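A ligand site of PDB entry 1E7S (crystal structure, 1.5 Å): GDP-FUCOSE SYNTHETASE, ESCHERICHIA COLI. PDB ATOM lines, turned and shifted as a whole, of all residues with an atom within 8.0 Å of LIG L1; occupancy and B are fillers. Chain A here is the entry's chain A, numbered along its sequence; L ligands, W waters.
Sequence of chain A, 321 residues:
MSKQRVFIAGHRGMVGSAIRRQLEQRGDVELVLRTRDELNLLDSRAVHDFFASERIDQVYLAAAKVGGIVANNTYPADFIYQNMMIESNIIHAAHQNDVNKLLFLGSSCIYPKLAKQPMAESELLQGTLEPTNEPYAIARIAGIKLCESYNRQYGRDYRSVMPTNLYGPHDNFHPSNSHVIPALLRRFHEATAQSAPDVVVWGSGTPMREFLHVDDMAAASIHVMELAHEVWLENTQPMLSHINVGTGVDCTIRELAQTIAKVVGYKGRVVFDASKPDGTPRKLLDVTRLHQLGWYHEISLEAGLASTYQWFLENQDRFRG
The backbone NH (N) of Val 70 sits at hydrogen-bond distance from an oxygen (O1) of LIG L1 (2.6 Å). N of Gly 68 lies within hydrogen-bond range of O3 of LIG L1 (2.7 Å). N of Ala 71 is in hydrogen-bond range of O2 of LIG L1, 2.8 Å away. The backbone NH (N) of Ile 69 is in hydrogen-bond range of an oxygen (O1) of LIG L1 (3.1 Å). The side-chain amide oxygen (OD1) of Asn 177 lies close to an oxygen (O14) of LG2 L2 (3.4 Å). ND1 of His 179 lies close to O14 of LG2 L2.
An oxygen (O3) of LIG L1 is in hydrogen-bond range of a nitrogen (N7) of LG2 L2, at 3.2 Å.
The backbone carbonyl oxygen (O) of Val 70 lies within hydrogen-bond range of the side-chain hydroxyl (OG1) of Thr 74, at 2.7 Å. The backbone carbonyl oxygen of Gly 68 sits at hydrogen-bond distance from the side-chain amide nitrogen of Asn 72 (3.0 Å). The backbone NH (N) of Ile 69 lies within hydrogen-bond range of the side-chain hydroxyl (OG) of Ser 178, 3.0 Å away. The side-chain amide nitrogen (ND2) of Asn 73 sits at hydrogen-bond distance from the backbone carbonyl oxygen (O) of Ile 69. O of Gly 67 sits at hydrogen-bond distance from ND2 of Asn 72, 3.1 Å away.
Residues that only touch LIG L1: Gly 67 (3.5 Å) and Ser 178 (3.4 Å). The nearest printed residue that does not touch LIG L1 is Ser 176 (4.1 Å).
Water W3 bridges O5 of LIG L1 (2.5 Å) and OG of Ser 176 (3.0 Å).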
ATOM      1  N   LYS A  65      29.172  23.979 -26.856  1.00  0.00           N
ATOM      2  CA  LYS A  65      28.698  25.353 -26.613  1.00  0.00           C
ATOM      3  C   LYS A  65      27.371  25.510 -27.362  1.00  0.00           C
ATOM      4  O   LYS A  65      27.362  25.403 -28.588  1.00  0.00           O
ATOM      5  CB  LYS A  65      29.788  26.308 -27.124  1.00  0.00           C
ATOM      6  CG  LYS A  65      29.402  27.751 -27.164  1.00  0.00           C
ATOM      7  CD  LYS A  65      28.885  28.246 -25.841  1.00  0.00           C
ATOM      8  CE  LYS A  65      28.827  29.804 -25.938  1.00  0.00           C
ATOM      9  NZ  LYS A  65      28.315  30.415 -24.698  1.00  0.00           N
ATOM     10  N   VAL A  66      26.285  25.598 -26.599  1.00  0.00           N
ATOM     11  CA  VAL A  66      24.923  25.549 -27.144  1.00  0.00           C
ATOM     12  C   VAL A  66      24.150  26.719 -26.568  1.00  0.00           C
ATOM     13  O   VAL A  66      24.377  27.168 -25.438  1.00  0.00           O
ATOM     14  CB  VAL A  66      24.217  24.239 -26.727  1.00  0.00           C
ATOM     15  CG1 VAL A  66      22.839  24.077 -27.337  1.00  0.00           C
ATOM     16  CG2 VAL A  66      25.068  23.058 -27.211  1.00  0.00           C
ATOM     17  N   GLY A  67      23.295  27.292 -27.436  1.00  0.00           N
ATOM     18  CA  GLY A  67      22.511  28.443 -27.020  1.00  0.00           C
ATOM     19  C   GLY A  67      21.296  28.619 -27.944  1.00  0.00           C
ATOM     20  O   GLY A  67      21.085  27.825 -28.872  1.00  0.00           O
ATOM     21  N   GLY A  68      20.553  29.684 -27.682  1.00  0.00           N
ATOM     22  CA  GLY A  68      19.369  29.992 -28.457  1.00  0.00           C
ATOM     23  C   GLY A  68      19.605  30.991 -29.568  1.00  0.00           C
ATOM     24  O   GLY A  68      20.732  31.189 -30.041  1.00  0.00           O
ATOM     25  N   ILE A  69      18.478  31.566 -30.069  1.00  0.00           N
ATOM     26  CA  ILE A  69      18.595  32.423 -31.238  1.00  0.00           C
ATOM     27  C   ILE A  69      19.427  33.672 -31.048  1.00  0.00           C
ATOM     28  O   ILE A  69      20.249  34.064 -31.905  1.00  0.00           O
ATOM     29  CB  ILE A  69      17.143  32.861 -31.611  1.00  0.00           C
ATOM     30  CG1 ILE A  69      16.362  31.667 -32.159  1.00  0.00           C
ATOM     31  CG2 ILE A  69      17.185  33.987 -32.642  1.00  0.00           C
ATOM     32  CD1 ILE A  69      14.927  31.999 -32.516  1.00  0.00           C
ATOM     33  N   VAL A  70      19.227  34.363 -29.934  1.00  0.00           N
ATOM     34  CA  VAL A  70      19.996  35.561 -29.633  1.00  0.00           C
ATOM     35  C   VAL A  70      21.471  35.173 -29.488  1.00  0.00           C
ATOM     36  O   VAL A  70      22.297  35.873 -30.118  1.00  0.00           O
ATOM     37  CB  VAL A  70      19.521  36.310 -28.394  1.00  0.00           C
ATOM     38  CG1 VAL A  70      20.467  37.433 -28.028  1.00  0.00           C
ATOM     39  CG2 VAL A  70      18.104  36.858 -28.548  1.00  0.00           C
ATOM     40  N   ALA A  71      21.785  34.127 -28.728  1.00  0.00           N
ATOM     41  CA  ALA A  71      23.187  33.803 -28.511  1.00  0.00           C
ATOM     42  C   ALA A  71      23.847  33.431 -29.843  1.00  0.00           C
ATOM     43  O   ALA A  71      24.978  33.880 -30.114  1.00  0.00           O
ATOM     44  CB  ALA A  71      23.291  32.646 -27.558  1.00  0.00           C
ATOM     45  N   ASN A  72      23.204  32.614 -30.668  1.00  0.00           N
ATOM     46  CA  ASN A  72      23.830  32.166 -31.903  1.00  0.00           C
ATOM     47  C   ASN A  72      24.104  33.368 -32.833  1.00  0.00           C
ATOM     48  O   ASN A  72      25.078  33.301 -33.582  1.00  0.00           O
ATOM     49  CB  ASN A  72      23.013  31.087 -32.593  1.00  0.00           C
ATOM     50  CG  ASN A  72      23.387  29.689 -32.110  1.00  0.00           C
ATOM     51  OD1 ASN A  72      24.296  29.067 -32.666  1.00  0.00           O
ATOM     52  ND2 ASN A  72      22.725  29.224 -31.056  1.00  0.00           N
ATOM     53  N   ASN A  73      23.221  34.354 -32.898  1.00  0.00           N
ATOM     54  CA  ASN A  73      23.471  35.496 -33.757  1.00  0.00           C
ATOM     55  C   ASN A  73      24.467  36.483 -33.148  1.00  0.00           C
ATOM     56  O   ASN A  73      25.019  37.302 -33.902  1.00  0.00           O
ATOM     57  CB  ASN A  73      22.163  36.281 -34.021  1.00  0.00           C
ATOM     58  CG  ASN A  73      21.269  35.579 -35.037  1.00  0.00           C
ATOM     59  OD1 ASN A  73      21.682  35.506 -36.198  1.00  0.00           O
ATOM     60  ND2 ASN A  73      20.112  35.092 -34.707  1.00  0.00           N
ATOM     61  N   THR A  74      24.569  36.530 -31.828  1.00  0.00           N
ATOM     62  CA  THR A  74      25.383  37.510 -31.131  1.00  0.00           C
ATOM     63  C   THR A  74      26.834  37.077 -30.974  1.00  0.00           C
ATOM     64  O   THR A  74      27.724  37.930 -31.028  1.00  0.00           O
ATOM     65  CB  THR A  74      24.734  37.847 -29.780  1.00  0.00           C
ATOM     66  OG1 THR A  74      23.395  38.359 -29.999  1.00  0.00           O
ATOM     67  CG2 THR A  74      25.542  38.809 -28.931  1.00  0.00           C
ATOM     68  N   TYR A  75      27.033  35.781 -30.776  1.00  0.00           N
ATOM     69  CA  TYR A  75      28.382  35.262 -30.538  1.00  0.00           C
ATOM     70  C   TYR A  75      28.723  34.144 -31.505  1.00  0.00           C
ATOM     71  O   TYR A  75      29.149  33.029 -31.134  1.00  0.00           O
ATOM     72  CB  TYR A  75      28.454  34.709 -29.103  1.00  0.00           C
ATOM     73  CG  TYR A  75      28.008  35.667 -28.005  1.00  0.00           C
ATOM     74  CD1 TYR A  75      28.886  36.672 -27.577  1.00  0.00           C
ATOM     75  CD2 TYR A  75      26.752  35.607 -27.419  1.00  0.00           C
ATOM     76  CE1 TYR A  75      28.529  37.554 -26.597  1.00  0.00           C
ATOM     77  CE2 TYR A  75      26.379  36.502 -26.452  1.00  0.00           C
ATOM     78  CZ  TYR A  75      27.253  37.493 -26.048  1.00  0.00           C
ATOM     79  OH  TYR A  75      26.927  38.420 -25.074  1.00  0.00           O
ATOM     80  N   PHE A  79      30.420  30.056 -31.064  1.00  0.00           N
ATOM     81  CA  PHE A  79      29.747  28.801 -31.406  1.00  0.00           C
ATOM     82  C   PHE A  79      30.505  27.974 -32.429  1.00  0.00           C
ATOM     83  O   PHE A  79      30.509  26.745 -32.306  1.00  0.00           O
ATOM     84  CB  PHE A  79      28.322  29.116 -31.902  1.00  0.00           C
ATOM     85  CG  PHE A  79      27.410  29.383 -30.750  1.00  0.00           C
ATOM     86  CD1 PHE A  79      26.825  28.329 -30.038  1.00  0.00           C
ATOM     87  CD2 PHE A  79      27.145  30.661 -30.345  1.00  0.00           C
ATOM     88  CE1 PHE A  79      26.049  28.571 -28.926  1.00  0.00           C
ATOM     89  CE2 PHE A  79      26.364  30.903 -29.257  1.00  0.00           C
ATOM     90  CZ  PHE A  79      25.745  29.889 -28.554  1.00  0.00           C
ATOM     91  N   THR A 132      20.798  31.955 -38.698  1.00  0.00           N
ATOM     92  CA  THR A 132      20.970  32.145 -37.240  1.00  0.00           C
ATOM     93  C   THR A 132      21.990  31.143 -36.711  1.00  0.00           C
ATOM     94  O   THR A 132      22.738  31.526 -35.803  1.00  0.00           O
ATOM     95  CB  THR A 132      19.618  32.004 -36.537  1.00  0.00           C
ATOM     96  OG1 THR A 132      18.915  33.232 -36.742  1.00  0.00           O
ATOM     97  CG2 THR A 132      19.709  31.713 -35.031  1.00  0.00           C
ATOM     98  N   ASN A 172      16.750  25.152 -19.419  1.00  0.00           N
ATOM     99  CA  ASN A 172      16.701  26.541 -18.954  1.00  0.00           C
ATOM    100  C   ASN A 172      15.274  27.064 -18.953  1.00  0.00           C
ATOM    101  O   ASN A 172      14.746  27.458 -20.023  1.00  0.00           O
ATOM    102  CB  ASN A 172      17.596  27.380 -19.878  1.00  0.00           C
ATOM    103  CG  ASN A 172      17.649  28.857 -19.553  1.00  0.00           C
ATOM    104  OD1 ASN A 172      18.141  29.674 -20.345  1.00  0.00           O
ATOM    105  ND2 ASN A 172      17.192  29.232 -18.359  1.00  0.00           N
ATOM    106  N   HIS A 174      13.369  29.775 -18.366  1.00  0.00           N
ATOM    107  CA  HIS A 174      13.351  31.224 -18.268  1.00  0.00           C
ATOM    108  C   HIS A 174      12.427  31.707 -19.378  1.00  0.00           C
ATOM    109  O   HIS A 174      12.409  31.114 -20.458  1.00  0.00           O
ATOM    110  CB  HIS A 174      14.768  31.768 -18.423  1.00  0.00           C
ATOM    111  CG  HIS A 174      14.896  33.223 -18.145  1.00  0.00           C
ATOM    112  ND1 HIS A 174      14.633  34.171 -19.111  1.00  0.00           N
ATOM    113  CD2 HIS A 174      15.209  33.897 -17.001  1.00  0.00           C
ATOM    114  CE1 HIS A 174      14.837  35.384 -18.585  1.00  0.00           C
ATOM    115  NE2 HIS A 174      15.168  35.241 -17.307  1.00  0.00           N
ATOM    116  N   SER A 176      12.528  34.027 -21.319  1.00  0.00           N
ATOM    117  CA  SER A 176      13.214  34.475 -22.498  1.00  0.00           C
ATOM    118  C   SER A 176      13.868  33.418 -23.375  1.00  0.00           C
ATOM    119  O   SER A 176      14.360  33.760 -24.464  1.00  0.00           O
ATOM    120  CB  SER A 176      14.338  35.468 -22.109  1.00  0.00           C
ATOM    121  OG  SER A 176      15.468  34.758 -21.607  1.00  0.00           O
ATOM    122  N   ASN A 177      13.752  32.154 -22.967  1.00  0.00           N
ATOM    123  CA  ASN A 177      14.405  31.073 -23.740  1.00  0.00           C
ATOM    124  C   ASN A 177      13.748  31.069 -25.107  1.00  0.00           C
ATOM    125  O   ASN A 177      12.508  31.069 -25.246  1.00  0.00           O
ATOM    126  CB  ASN A 177      14.237  29.761 -22.944  1.00  0.00           C
ATOM    127  CG  ASN A 177      15.083  28.617 -23.498  1.00  0.00           C
ATOM    128  OD1 ASN A 177      15.340  28.492 -24.696  1.00  0.00           O
ATOM    129  ND2 ASN A 177      15.475  27.667 -22.664  1.00  0.00           N
ATOM    130  N   SER A 178      14.541  30.948 -26.183  1.00  0.00           N
ATOM    131  CA  SER A 178      13.980  30.808 -27.528  1.00  0.00           C
ATOM    132  C   SER A 178      13.435  29.418 -27.837  1.00  0.00           C
ATOM    133  O   SER A 178      12.772  29.242 -28.842  1.00  0.00           O
ATOM    134  CB  SER A 178      14.929  31.264 -28.620  1.00  0.00           C
ATOM    135  OG  SER A 178      16.107  30.504 -28.597  1.00  0.00           O
ATOM    136  N   HIS A 179      13.701  28.417 -27.030  1.00  0.00           N
ATOM    137  CA  HIS A 179      13.146  27.087 -27.157  1.00  0.00           C
ATOM    138  C   HIS A 179      11.745  27.079 -26.539  1.00  0.00           C
ATOM    139  O   HIS A 179      11.561  27.437 -25.369  1.00  0.00           O
ATOM    140  CB  HIS A 179      14.007  26.008 -26.503  1.00  0.00           C
ATOM    141  CG  HIS A 179      15.385  25.870 -27.019  1.00  0.00           C
ATOM    142  ND1 HIS A 179      16.433  26.637 -26.556  1.00  0.00           N
ATOM    143  CD2 HIS A 179      15.869  25.174 -28.067  1.00  0.00           C
ATOM    144  CE1 HIS A 179      17.524  26.356 -27.242  1.00  0.00           C
ATOM    145  NE2 HIS A 179      17.215  25.506 -28.181  1.00  0.00           N
HETATM  146  C1  LIG L   1      18.300  32.959 -27.076  1.00  0.00           C
HETATM  147  O1  LIG L   1      17.756  33.645 -27.942  1.00  0.00           O
HETATM  148  C2  LIG L   1      17.762  32.237 -26.182  1.00  0.00           C
HETATM  149  O2  LIG L   1      19.849  32.641 -27.286  1.00  0.00           O
HETATM  150  P1  LIG L   1      20.207  32.447 -25.861  1.00  0.00           P
HETATM  151  O3  LIG L   1      21.115  31.360 -25.643  1.00  0.00           O
HETATM  152  O4  LIG L   1      20.977  33.632 -25.560  1.00  0.00           O
HETATM  153  O5  LIG L   1      19.018  32.514 -24.816  1.00  0.00           O
HETATM  154  P1  LG2 L   2      24.391  21.940 -22.478  1.00  0.00           P
HETATM  155  O1  LG2 L   2      24.843  23.332 -22.533  1.00  0.00           O
HETATM  156  O2  LG2 L   2      23.223  21.671 -21.541  1.00  0.00           O
HETATM  157  O3  LG2 L   2      25.528  20.965 -22.129  1.00  0.00           O
HETATM  158  C1  LG2 L   2      26.854  21.185 -22.694  1.00  0.00           C
HETATM  159  C2  LG2 L   2      27.841  20.742 -21.550  1.00  0.00           C
HETATM  160  O4  LG2 L   2      29.189  20.922 -22.135  1.00  0.00           O
HETATM  161  C3  LG2 L   2      27.807  21.739 -20.348  1.00  0.00           C
HETATM  162  O5  LG2 L   2      27.884  21.007 -19.139  1.00  0.00           O
HETATM  163  C4  LG2 L   2      29.060  22.606 -20.563  1.00  0.00           C
HETATM  164  O6  LG2 L   2      29.673  23.072 -19.345  1.00  0.00           O
HETATM  165  C5  LG2 L   2      29.982  21.582 -21.171  1.00  0.00           C
HETATM  166  N1  LG2 L   2      31.097  22.189 -21.865  1.00  0.00           N
HETATM  167  C6  LG2 L   2      31.021  23.163 -22.826  1.00  0.00           C
HETATM  168  N2  LG2 L   2      32.230  23.604 -23.120  1.00  0.00           N
HETATM  169  C7  LG2 L   2      33.121  22.934 -22.284  1.00  0.00           C
HETATM  170  C8  LG2 L   2      34.533  23.016 -22.110  1.00  0.00           C
HETATM  171  N3  LG2 L   2      35.293  23.946 -22.754  1.00  0.00           N
HETATM  172  N4  LG2 L   2      35.105  22.168 -21.223  1.00  0.00           N
HETATM  173  C9  LG2 L   2      34.326  21.293 -20.534  1.00  0.00           C
HETATM  174  N5  LG2 L   2      32.974  21.226 -20.570  1.00  0.00           N
HETATM  175  C10 LG2 L   2      32.429  21.986 -21.567  1.00  0.00           C
HETATM  176  O7  LG2 L   2      24.035  21.524 -23.877  1.00  0.00           O
HETATM  177  P2  LG2 L   2      23.222  20.230 -24.504  1.00  0.00           P
HETATM  178  O8  LG2 L   2      23.156  19.174 -23.450  1.00  0.00           O
HETATM  179  O9  LG2 L   2      23.794  19.832 -25.874  1.00  0.00           O
HETATM  180  O10 LG2 L   2      21.820  20.835 -24.618  1.00  0.00           O
HETATM  181  C11 LG2 L   2      20.732  20.045 -25.112  1.00  0.00           C
HETATM  182  C12 LG2 L   2      19.529  20.948 -25.245  1.00  0.00           C
HETATM  183  O11 LG2 L   2      19.445  21.665 -24.007  1.00  0.00           O
HETATM  184  C13 LG2 L   2      19.724  22.138 -26.222  1.00  0.00           C
HETATM  185  O12 LG2 L   2      19.334  21.568 -27.479  1.00  0.00           O
HETATM  186  C14 LG2 L   2      18.477  22.945 -25.728  1.00  0.00           C
HETATM  187  O13 LG2 L   2      17.296  22.121 -25.951  1.00  0.00           O
HETATM  188  C15 LG2 L   2      18.793  22.897 -24.280  1.00  0.00           C
HETATM  189  N6  LG2 L   2      19.757  23.935 -24.131  1.00  0.00           N
HETATM  190  C16 LG2 L   2      19.350  25.247 -24.388  1.00  0.00           C
HETATM  191  C17 LG2 L   2      20.208  26.340 -24.188  1.00  0.00           C
HETATM  192  C18 LG2 L   2      19.800  27.795 -24.493  1.00  0.00           C
HETATM  193  O14 LG2 L   2      18.709  27.965 -25.113  1.00  0.00           O
HETATM  194  N7  LG2 L   2      20.592  28.783 -23.903  1.00  0.00           N
HETATM  195  C19 LG2 L   2      21.470  26.098 -23.626  1.00  0.00           C
HETATM  196  C20 LG2 L   2      21.868  24.750 -23.331  1.00  0.00           C
HETATM  197  C21 LG2 L   2      20.929  23.694 -23.548  1.00  0.00           C
HETATM  198  P3  LG2 L   2      29.521  24.554 -18.893  1.00  0.00           P
HETATM  199  O15 LG2 L   2      30.334  24.621 -17.635  1.00  0.00           O
HETATM  200  O16 LG2 L   2      29.900  25.478 -20.049  1.00  0.00           O
HETATM  201  O17 LG2 L   2      28.091  24.833 -18.777  1.00  0.00           O
HETATM  202  O   HOH W   1      19.298  35.815 -24.822  1.00  0.00           O
HETATM  203  O   HOH W   2      23.410  31.408 -23.977  1.00  0.00           O
HETATM  204  O   HOH W   3      17.550  33.081 -22.856  1.00  0.00           O
HETATM  205  O   HOH W   4      22.882  35.709 -25.684  1.00  0.00           O
